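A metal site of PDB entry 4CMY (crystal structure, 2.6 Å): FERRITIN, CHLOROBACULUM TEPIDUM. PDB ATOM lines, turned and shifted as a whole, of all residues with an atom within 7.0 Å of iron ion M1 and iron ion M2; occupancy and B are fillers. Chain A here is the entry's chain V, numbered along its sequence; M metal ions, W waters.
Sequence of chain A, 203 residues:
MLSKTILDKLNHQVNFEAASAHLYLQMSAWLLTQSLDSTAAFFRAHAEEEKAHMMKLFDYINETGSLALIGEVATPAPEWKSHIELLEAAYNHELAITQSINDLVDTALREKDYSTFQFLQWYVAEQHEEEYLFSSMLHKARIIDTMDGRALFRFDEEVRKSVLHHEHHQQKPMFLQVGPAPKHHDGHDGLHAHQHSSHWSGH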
ATOM      1  N   GLN A  13      24.708  32.948  20.762  1.00  0.00           N
ATOM      2  CA  GLN A  13      23.901  31.796  20.347  1.00  0.00           C
ATOM      3  C   GLN A  13      22.510  32.216  19.872  1.00  0.00           C
ATOM      4  O   GLN A  13      22.031  31.727  18.854  1.00  0.00           O
ATOM      5  CB  GLN A  13      23.756  30.812  21.496  1.00  0.00           C
ATOM      6  CG  GLN A  13      23.315  29.458  21.065  1.00  0.00           C
ATOM      7  CD  GLN A  13      24.343  28.764  20.183  1.00  0.00           C
ATOM      8  OE1 GLN A  13      25.536  28.911  20.373  1.00  0.00           O
ATOM      9  NE2 GLN A  13      23.870  27.996  19.210  1.00  0.00           N
ATOM     10  N   PHE A  16      23.185  33.283  16.469  1.00  0.00           N
ATOM     11  CA  PHE A  16      23.505  32.110  15.616  1.00  0.00           C
ATOM     12  C   PHE A  16      22.224  31.387  15.195  1.00  0.00           C
ATOM     13  O   PHE A  16      22.080  30.970  14.062  1.00  0.00           O
ATOM     14  CB  PHE A  16      24.431  31.165  16.422  1.00  0.00           C
ATOM     15  CG  PHE A  16      25.316  30.248  15.587  1.00  0.00           C
ATOM     16  CD1 PHE A  16      25.301  30.229  14.217  1.00  0.00           C
ATOM     17  CD2 PHE A  16      26.220  29.430  16.229  1.00  0.00           C
ATOM     18  CE1 PHE A  16      26.152  29.412  13.501  1.00  0.00           C
ATOM     19  CE2 PHE A  16      27.059  28.594  15.523  1.00  0.00           C
ATOM     20  CZ  PHE A  16      27.042  28.586  14.161  1.00  0.00           C
ATOM     21  N   GLU A  17      21.295  31.186  16.139  1.00  0.00           N
ATOM     22  CA  GLU A  17      20.044  30.504  15.822  1.00  0.00           C
ATOM     23  C   GLU A  17      19.239  31.365  14.847  1.00  0.00           C
ATOM     24  O   GLU A  17      18.677  30.841  13.892  1.00  0.00           O
ATOM     25  CB  GLU A  17      19.235  30.184  17.090  1.00  0.00           C
ATOM     26  CG  GLU A  17      19.950  29.302  18.085  1.00  0.00           C
ATOM     27  CD  GLU A  17      20.149  27.822  17.666  1.00  0.00           C
ATOM     28  OE1 GLU A  17      19.399  27.311  16.795  1.00  0.00           O
ATOM     29  OE2 GLU A  17      21.012  27.162  18.305  1.00  0.00           O
ATOM     30  N   SER A  20      20.588  30.872  11.520  1.00  0.00           N
ATOM     31  CA  SER A  20      20.226  29.543  10.981  1.00  0.00           C
ATOM     32  C   SER A  20      18.863  29.562  10.352  1.00  0.00           C
ATOM     33  O   SER A  20      18.660  29.004   9.305  1.00  0.00           O
ATOM     34  CB  SER A  20      20.243  28.494  12.084  1.00  0.00           C
ATOM     35  OG  SER A  20      21.506  28.519  12.741  1.00  0.00           O
ATOM     36  N   TYR A  24      18.253  28.771   6.402  1.00  0.00           N
ATOM     37  CA  TYR A  24      17.389  27.697   5.912  1.00  0.00           C
ATOM     38  C   TYR A  24      16.257  28.236   5.072  1.00  0.00           C
ATOM     39  O   TYR A  24      15.837  27.608   4.128  1.00  0.00           O
ATOM     40  CB  TYR A  24      16.885  26.835   7.087  1.00  0.00           C
ATOM     41  CG  TYR A  24      17.980  26.033   7.816  1.00  0.00           C
ATOM     42  CD1 TYR A  24      19.160  25.674   7.196  1.00  0.00           C
ATOM     43  CD2 TYR A  24      17.804  25.617   9.136  1.00  0.00           C
ATOM     44  CE1 TYR A  24      20.132  24.963   7.864  1.00  0.00           C
ATOM     45  CE2 TYR A  24      18.759  24.919   9.796  1.00  0.00           C
ATOM     46  CZ  TYR A  24      19.928  24.594   9.165  1.00  0.00           C
ATOM     47  OH  TYR A  24      20.930  23.905   9.812  1.00  0.00           O
ATOM     48  N   HIS A  46      11.987  23.833   8.811  1.00  0.00           N
ATOM     49  CA  HIS A  46      13.052  23.802   9.764  1.00  0.00           C
ATOM     50  C   HIS A  46      13.525  25.204  10.164  1.00  0.00           C
ATOM     51  O   HIS A  46      14.077  25.390  11.245  1.00  0.00           O
ATOM     52  CB  HIS A  46      14.223  22.974   9.264  1.00  0.00           C
ATOM     53  CG  HIS A  46      14.947  22.337  10.364  1.00  0.00           C
ATOM     54  ND1 HIS A  46      14.462  21.221  11.004  1.00  0.00           N
ATOM     55  CD2 HIS A  46      16.050  22.719  11.055  1.00  0.00           C
ATOM     56  CE1 HIS A  46      15.244  20.920  12.013  1.00  0.00           C
ATOM     57  NE2 HIS A  46      16.216  21.805  12.063  1.00  0.00           N
ATOM     58  N   GLU A  49      11.771  25.885  13.218  1.00  0.00           N
ATOM     59  CA  GLU A  49      12.389  25.231  14.365  1.00  0.00           C
ATOM     60  C   GLU A  49      13.544  26.052  14.900  1.00  0.00           C
ATOM     61  O   GLU A  49      13.682  26.189  16.111  1.00  0.00           O
ATOM     62  CB  GLU A  49      12.885  23.825  14.014  1.00  0.00           C
ATOM     63  CG  GLU A  49      11.777  22.790  13.943  1.00  0.00           C
ATOM     64  CD  GLU A  49      11.263  22.426  15.325  1.00  0.00           C
ATOM     65  OE1 GLU A  49      12.053  22.269  16.314  1.00  0.00           O
ATOM     66  OE2 GLU A  49      10.020  22.351  15.414  1.00  0.00           O
ATOM     67  N   GLU A  50      14.350  26.629  14.019  1.00  0.00           N
ATOM     68  CA  GLU A  50      15.464  27.422  14.479  1.00  0.00           C
ATOM     69  C   GLU A  50      14.987  28.683  15.179  1.00  0.00           C
ATOM     70  O   GLU A  50      15.627  29.154  16.100  1.00  0.00           O
ATOM     71  CB  GLU A  50      16.422  27.733  13.310  1.00  0.00           C
ATOM     72  CG  GLU A  50      17.069  26.482  12.678  1.00  0.00           C
ATOM     73  CD  GLU A  50      18.007  25.682  13.602  1.00  0.00           C
ATOM     74  OE1 GLU A  50      18.349  26.186  14.711  1.00  0.00           O
ATOM     75  OE2 GLU A  50      18.361  24.486  13.199  1.00  0.00           O
ATOM     76  N   LYS A  51      13.870  29.232  14.754  1.00  0.00           N
ATOM     77  CA  LYS A  51      13.272  30.390  15.400  1.00  0.00           C
ATOM     78  C   LYS A  51      12.856  30.049  16.784  1.00  0.00           C
ATOM     79  O   LYS A  51      13.072  30.828  17.679  1.00  0.00           O
ATOM     80  CB  LYS A  51      12.051  30.872  14.625  1.00  0.00           C
ATOM     81  CG  LYS A  51      11.982  32.353  14.311  1.00  0.00           C
ATOM     82  CD  LYS A  51      12.432  32.545  12.858  1.00  0.00           C
ATOM     83  CE  LYS A  51      12.843  33.955  12.441  1.00  0.00           C
ATOM     84  NZ  LYS A  51      13.794  34.084  11.294  1.00  0.00           N
ATOM     85  N   HIS A  53      14.322  27.766  18.634  1.00  0.00           N
ATOM     86  CA  HIS A  53      15.553  27.641  19.394  1.00  0.00           C
ATOM     87  C   HIS A  53      15.998  29.014  19.836  1.00  0.00           C
ATOM     88  O   HIS A  53      16.445  29.196  20.960  1.00  0.00           O
ATOM     89  CB  HIS A  53      16.679  27.012  18.587  1.00  0.00           C
ATOM     90  CG  HIS A  53      16.421  25.604  18.158  1.00  0.00           C
ATOM     91  ND1 HIS A  53      17.235  24.941  17.251  1.00  0.00           N
ATOM     92  CD2 HIS A  53      15.410  24.745  18.447  1.00  0.00           C
ATOM     93  CE1 HIS A  53      16.741  23.727  17.022  1.00  0.00           C
ATOM     94  NE2 HIS A  53      15.634  23.587  17.727  1.00  0.00           N
ATOM     95  N   MET A  54      15.903  29.968  18.931  1.00  0.00           N
ATOM     96  CA  MET A  54      16.293  31.325  19.233  1.00  0.00           C
ATOM     97  C   MET A  54      15.477  31.857  20.386  1.00  0.00           C
ATOM     98  O   MET A  54      16.029  32.467  21.309  1.00  0.00           O
ATOM     99  CB  MET A  54      16.146  32.201  17.990  1.00  0.00           C
ATOM    100  CG  MET A  54      16.476  33.671  18.229  1.00  0.00           C
ATOM    101  SD  MET A  54      15.991  34.719  16.850  1.00  0.00           S
ATOM    102  CE  MET A  54      14.240  34.820  17.178  1.00  0.00           C
ATOM    103  N   HIS A  93      26.960  23.329   9.041  1.00  0.00           N
ATOM    104  CA  HIS A  93      26.396  24.393   9.835  1.00  0.00           C
ATOM    105  C   HIS A  93      25.849  23.827  11.145  1.00  0.00           C
ATOM    106  O   HIS A  93      26.082  24.395  12.219  1.00  0.00           O
ATOM    107  CB  HIS A  93      25.313  25.118   9.046  1.00  0.00           C
ATOM    108  CG  HIS A  93      24.691  26.230   9.789  1.00  0.00           C
ATOM    109  ND1 HIS A  93      25.214  27.502   9.800  1.00  0.00           N
ATOM    110  CD2 HIS A  93      23.567  26.292  10.545  1.00  0.00           C
ATOM    111  CE1 HIS A  93      24.435  28.300  10.509  1.00  0.00           C
ATOM    112  NE2 HIS A  93      23.436  27.578  10.994  1.00  0.00           N
ATOM    113  N   GLU A  94      25.148  22.707  11.067  1.00  0.00           N
ATOM    114  CA  GLU A  94      24.635  22.071  12.277  1.00  0.00           C
ATOM    115  C   GLU A  94      25.764  21.568  13.172  1.00  0.00           C
ATOM    116  O   GLU A  94      25.661  21.684  14.397  1.00  0.00           O
ATOM    117  CB  GLU A  94      23.612  20.969  11.962  1.00  0.00           C
ATOM    118  CG  GLU A  94      22.236  21.519  11.509  1.00  0.00           C
ATOM    119  CD  GLU A  94      21.422  22.169  12.616  1.00  0.00           C
ATOM    120  OE1 GLU A  94      21.759  21.865  13.793  1.00  0.00           O
ATOM    121  OE2 GLU A  94      20.444  22.947  12.333  1.00  0.00           O
ATOM    122  N   ILE A  97      26.929  24.576  15.046  1.00  0.00           N
ATOM    123  CA  ILE A  97      26.005  24.944  16.108  1.00  0.00           C
ATOM    124  C   ILE A  97      26.284  24.036  17.292  1.00  0.00           C
ATOM    125  O   ILE A  97      26.355  24.510  18.430  1.00  0.00           O
ATOM    126  CB  ILE A  97      24.526  24.833  15.667  1.00  0.00           C
ATOM    127  CG1 ILE A  97      24.197  25.984  14.753  1.00  0.00           C
ATOM    128  CG2 ILE A  97      23.592  24.944  16.869  1.00  0.00           C
ATOM    129  CD1 ILE A  97      22.933  25.754  13.999  1.00  0.00           C
ATOM    130  N   ILE A 101      27.256  25.149  21.111  1.00  0.00           N
ATOM    131  CA  ILE A 101      26.511  24.726  22.292  1.00  0.00           C
ATOM    132  C   ILE A 101      27.459  24.026  23.277  1.00  0.00           C
ATOM    133  O   ILE A 101      27.414  24.295  24.468  1.00  0.00           O
ATOM    134  CB  ILE A 101      25.347  23.783  21.933  1.00  0.00           C
ATOM    135  CG1 ILE A 101      24.273  24.495  21.127  1.00  0.00           C
ATOM    136  CG2 ILE A 101      24.744  23.192  23.194  1.00  0.00           C
ATOM    137  CD1 ILE A 101      23.536  25.598  21.861  1.00  0.00           C
ATOM    138  N   TRP A 122      18.697  20.793  27.133  1.00  0.00           N
ATOM    139  CA  TRP A 122      17.720  20.732  26.084  1.00  0.00           C
ATOM    140  C   TRP A 122      18.382  20.868  24.710  1.00  0.00           C
ATOM    141  O   TRP A 122      18.091  20.088  23.811  1.00  0.00           O
ATOM    142  CB  TRP A 122      16.683  21.830  26.269  1.00  0.00           C
ATOM    143  CG  TRP A 122      15.571  21.670  25.331  1.00  0.00           C
ATOM    144  CD1 TRP A 122      14.450  20.935  25.543  1.00  0.00           C
ATOM    145  CD2 TRP A 122      15.462  22.230  24.001  1.00  0.00           C
ATOM    146  NE1 TRP A 122      13.616  21.016  24.435  1.00  0.00           N
ATOM    147  CE2 TRP A 122      14.220  21.799  23.471  1.00  0.00           C
ATOM    148  CE3 TRP A 122      16.265  23.060  23.224  1.00  0.00           C
ATOM    149  CZ2 TRP A 122      13.767  22.151  22.199  1.00  0.00           C
ATOM    150  CZ3 TRP A 122      15.827  23.424  21.962  1.00  0.00           C
ATOM    151  CH2 TRP A 122      14.583  22.965  21.457  1.00  0.00           C
ATOM    152  N   TYR A 123      19.286  21.844  24.562  1.00  0.00           N
ATOM    153  CA  TYR A 123      19.999  22.067  23.295  1.00  0.00           C
ATOM    154  C   TYR A 123      20.960  20.946  22.951  1.00  0.00           C
ATOM    155  O   TYR A 123      21.151  20.616  21.785  1.00  0.00           O
ATOM    156  CB  TYR A 123      20.779  23.411  23.288  1.00  0.00           C
ATOM    157  CG  TYR A 123      19.850  24.568  23.201  1.00  0.00           C
ATOM    158  CD1 TYR A 123      19.243  25.045  24.339  1.00  0.00           C
ATOM    159  CD2 TYR A 123      19.522  25.137  22.001  1.00  0.00           C
ATOM    160  CE1 TYR A 123      18.308  26.077  24.282  1.00  0.00           C
ATOM    161  CE2 TYR A 123      18.612  26.180  21.935  1.00  0.00           C
ATOM    162  CZ  TYR A 123      18.005  26.631  23.083  1.00  0.00           C
ATOM    163  OH  TYR A 123      17.101  27.647  23.064  1.00  0.00           O
ATOM    164  N   GLU A 126      18.785  18.361  21.595  1.00  0.00           N
ATOM    165  CA  GLU A 126      18.202  18.760  20.319  1.00  0.00           C
ATOM    166  C   GLU A 126      19.238  18.695  19.204  1.00  0.00           C
ATOM    167  O   GLU A 126      18.935  18.269  18.120  1.00  0.00           O
ATOM    168  CB  GLU A 126      17.605  20.161  20.403  1.00  0.00           C
ATOM    169  CG  GLU A 126      16.750  20.544  19.194  1.00  0.00           C
ATOM    170  CD  GLU A 126      15.377  19.844  19.117  1.00  0.00           C
ATOM    171  OE1 GLU A 126      14.941  19.169  20.093  1.00  0.00           O
ATOM    172  OE2 GLU A 126      14.727  20.032  18.037  1.00  0.00           O
ATOM    173  N   GLN A 127      20.482  19.036  19.503  1.00  0.00           N
ATOM    174  CA  GLN A 127      21.520  18.982  18.491  1.00  0.00           C
ATOM    175  C   GLN A 127      21.882  17.562  18.097  1.00  0.00           C
ATOM    176  O   GLN A 127      22.298  17.324  16.962  1.00  0.00           O
ATOM    177  CB  GLN A 127      22.758  19.782  18.897  1.00  0.00           C
ATOM    178  CG  GLN A 127      22.452  21.272  18.811  1.00  0.00           C
ATOM    179  CD  GLN A 127      22.135  21.725  17.414  1.00  0.00           C
ATOM    180  OE1 GLN A 127      21.119  22.407  17.176  1.00  0.00           O
ATOM    181  NE2 GLN A 127      22.980  21.332  16.460  1.00  0.00           N
ATOM    182  N   GLU A 130      19.326  16.939  15.547  1.00  0.00           N
ATOM    183  CA  GLU A 130      19.615  17.725  14.345  1.00  0.00           C
ATOM    184  C   GLU A 130      20.698  17.080  13.515  1.00  0.00           C
ATOM    185  O   GLU A 130      20.593  16.982  12.307  1.00  0.00           O
ATOM    186  CB  GLU A 130      20.077  19.145  14.695  1.00  0.00           C
ATOM    187  CG  GLU A 130      19.058  20.027  15.376  1.00  0.00           C
ATOM    188  CD  GLU A 130      18.111  20.677  14.399  1.00  0.00           C
ATOM    189  OE1 GLU A 130      18.445  21.801  13.869  1.00  0.00           O
ATOM    190  OE2 GLU A 130      17.050  20.048  14.167  1.00  0.00           O
ATOM    191  N   PHE A 134      20.164  15.755   9.636  1.00  0.00           N
ATOM    192  CA  PHE A 134      20.917  16.325   8.523  1.00  0.00           C
ATOM    193  C   PHE A 134      21.974  15.393   7.947  1.00  0.00           C
ATOM    194  O   PHE A 134      22.190  15.380   6.755  1.00  0.00           O
ATOM    195  CB  PHE A 134      21.523  17.685   8.898  1.00  0.00           C
ATOM    196  CG  PHE A 134      20.525  18.821   8.928  1.00  0.00           C
ATOM    197  CD1 PHE A 134      20.251  19.531   7.801  1.00  0.00           C
ATOM    198  CD2 PHE A 134      19.861  19.144  10.099  1.00  0.00           C
ATOM    199  CE1 PHE A 134      19.330  20.548   7.824  1.00  0.00           C
ATOM    200  CE2 PHE A 134      18.927  20.143  10.132  1.00  0.00           C
ATOM    201  CZ  PHE A 134      18.655  20.855   8.991  1.00  0.00           C
HETATM  202 FE    FE M   1      19.216  25.273  16.431  1.00  0.00          FE
HETATM  203 FE    FE M   2      19.601  23.441  14.206  1.00  0.00          FE
HETATM  204  O   HOH W   1      20.102  24.567  18.641  1.00  0.00           O
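Iron ion M1 is bound by the side-chain carboxylate (OE1) of Glu 17, 2.1 Å away.
OE1 of Glu 50 binds iron ion M1 (2.1 Å).
ND1 of His 53 binds iron ion M1.
Water W1 is bound to iron ion M1.
Iron ion M1 has four donor atoms within binding distance.
Iron ion M2 is bound by OE2 of Glu 50.
The side-chain carboxylate (OE1) of Glu 130 is bound to iron ion M2 (2.0 Å).
Iron ion M2 is bound by OE2 of Glu 94, at 2.1 Å.
Slightly farther from iron ion M2 lies the side-chain carboxylate (OE1) of Glu 94 (2.7 Å).
The side-chain carboxylate (OE2) of Glu 130 lies within hydrogen-bond range of a ring nitrogen (NE2) of His 46, 2.9 Å away.
OE2 of Glu 17 lies within hydrogen-bond range of NE2 of Gln 13 (3.1 Å).
The side-chain amide nitrogen (NE2) of Gln 127 sits at hydrogen-bond distance from the side-chain carboxylate (OE1) of Glu 94 (3.0 Å).
The side-chain carboxylate (OE2) of Glu 94 lies close to the side-chain hydroxyl (OH) of Tyr 24, at 2.7 Å.
The backbone carbonyl oxygen (O) of His 53 sits at hydrogen-bond distance from the side-chain hydroxyl (OH) of Tyr 123 (2.7 Å).
Gln 127 touches iron ion M2.
The nearest printed residue that does not touch iron ion M2 is His 53 (4.02 Å).
Water W1 lies within hydrogen-bond range of OE2 of Glu 17 (2.8 Å) and OE1 of Gln 127 (2.8 Å).
OE1 of Gln 127 touches iron ion M1 (3.5 Å).
Four residues have an atom within 4 Å of iron ion M1: Glu 17, Glu 50, His 53 and Gln 127.
The nearest printed residue that does not touch iron ion M1 is Glu 130 (4.4 Å).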
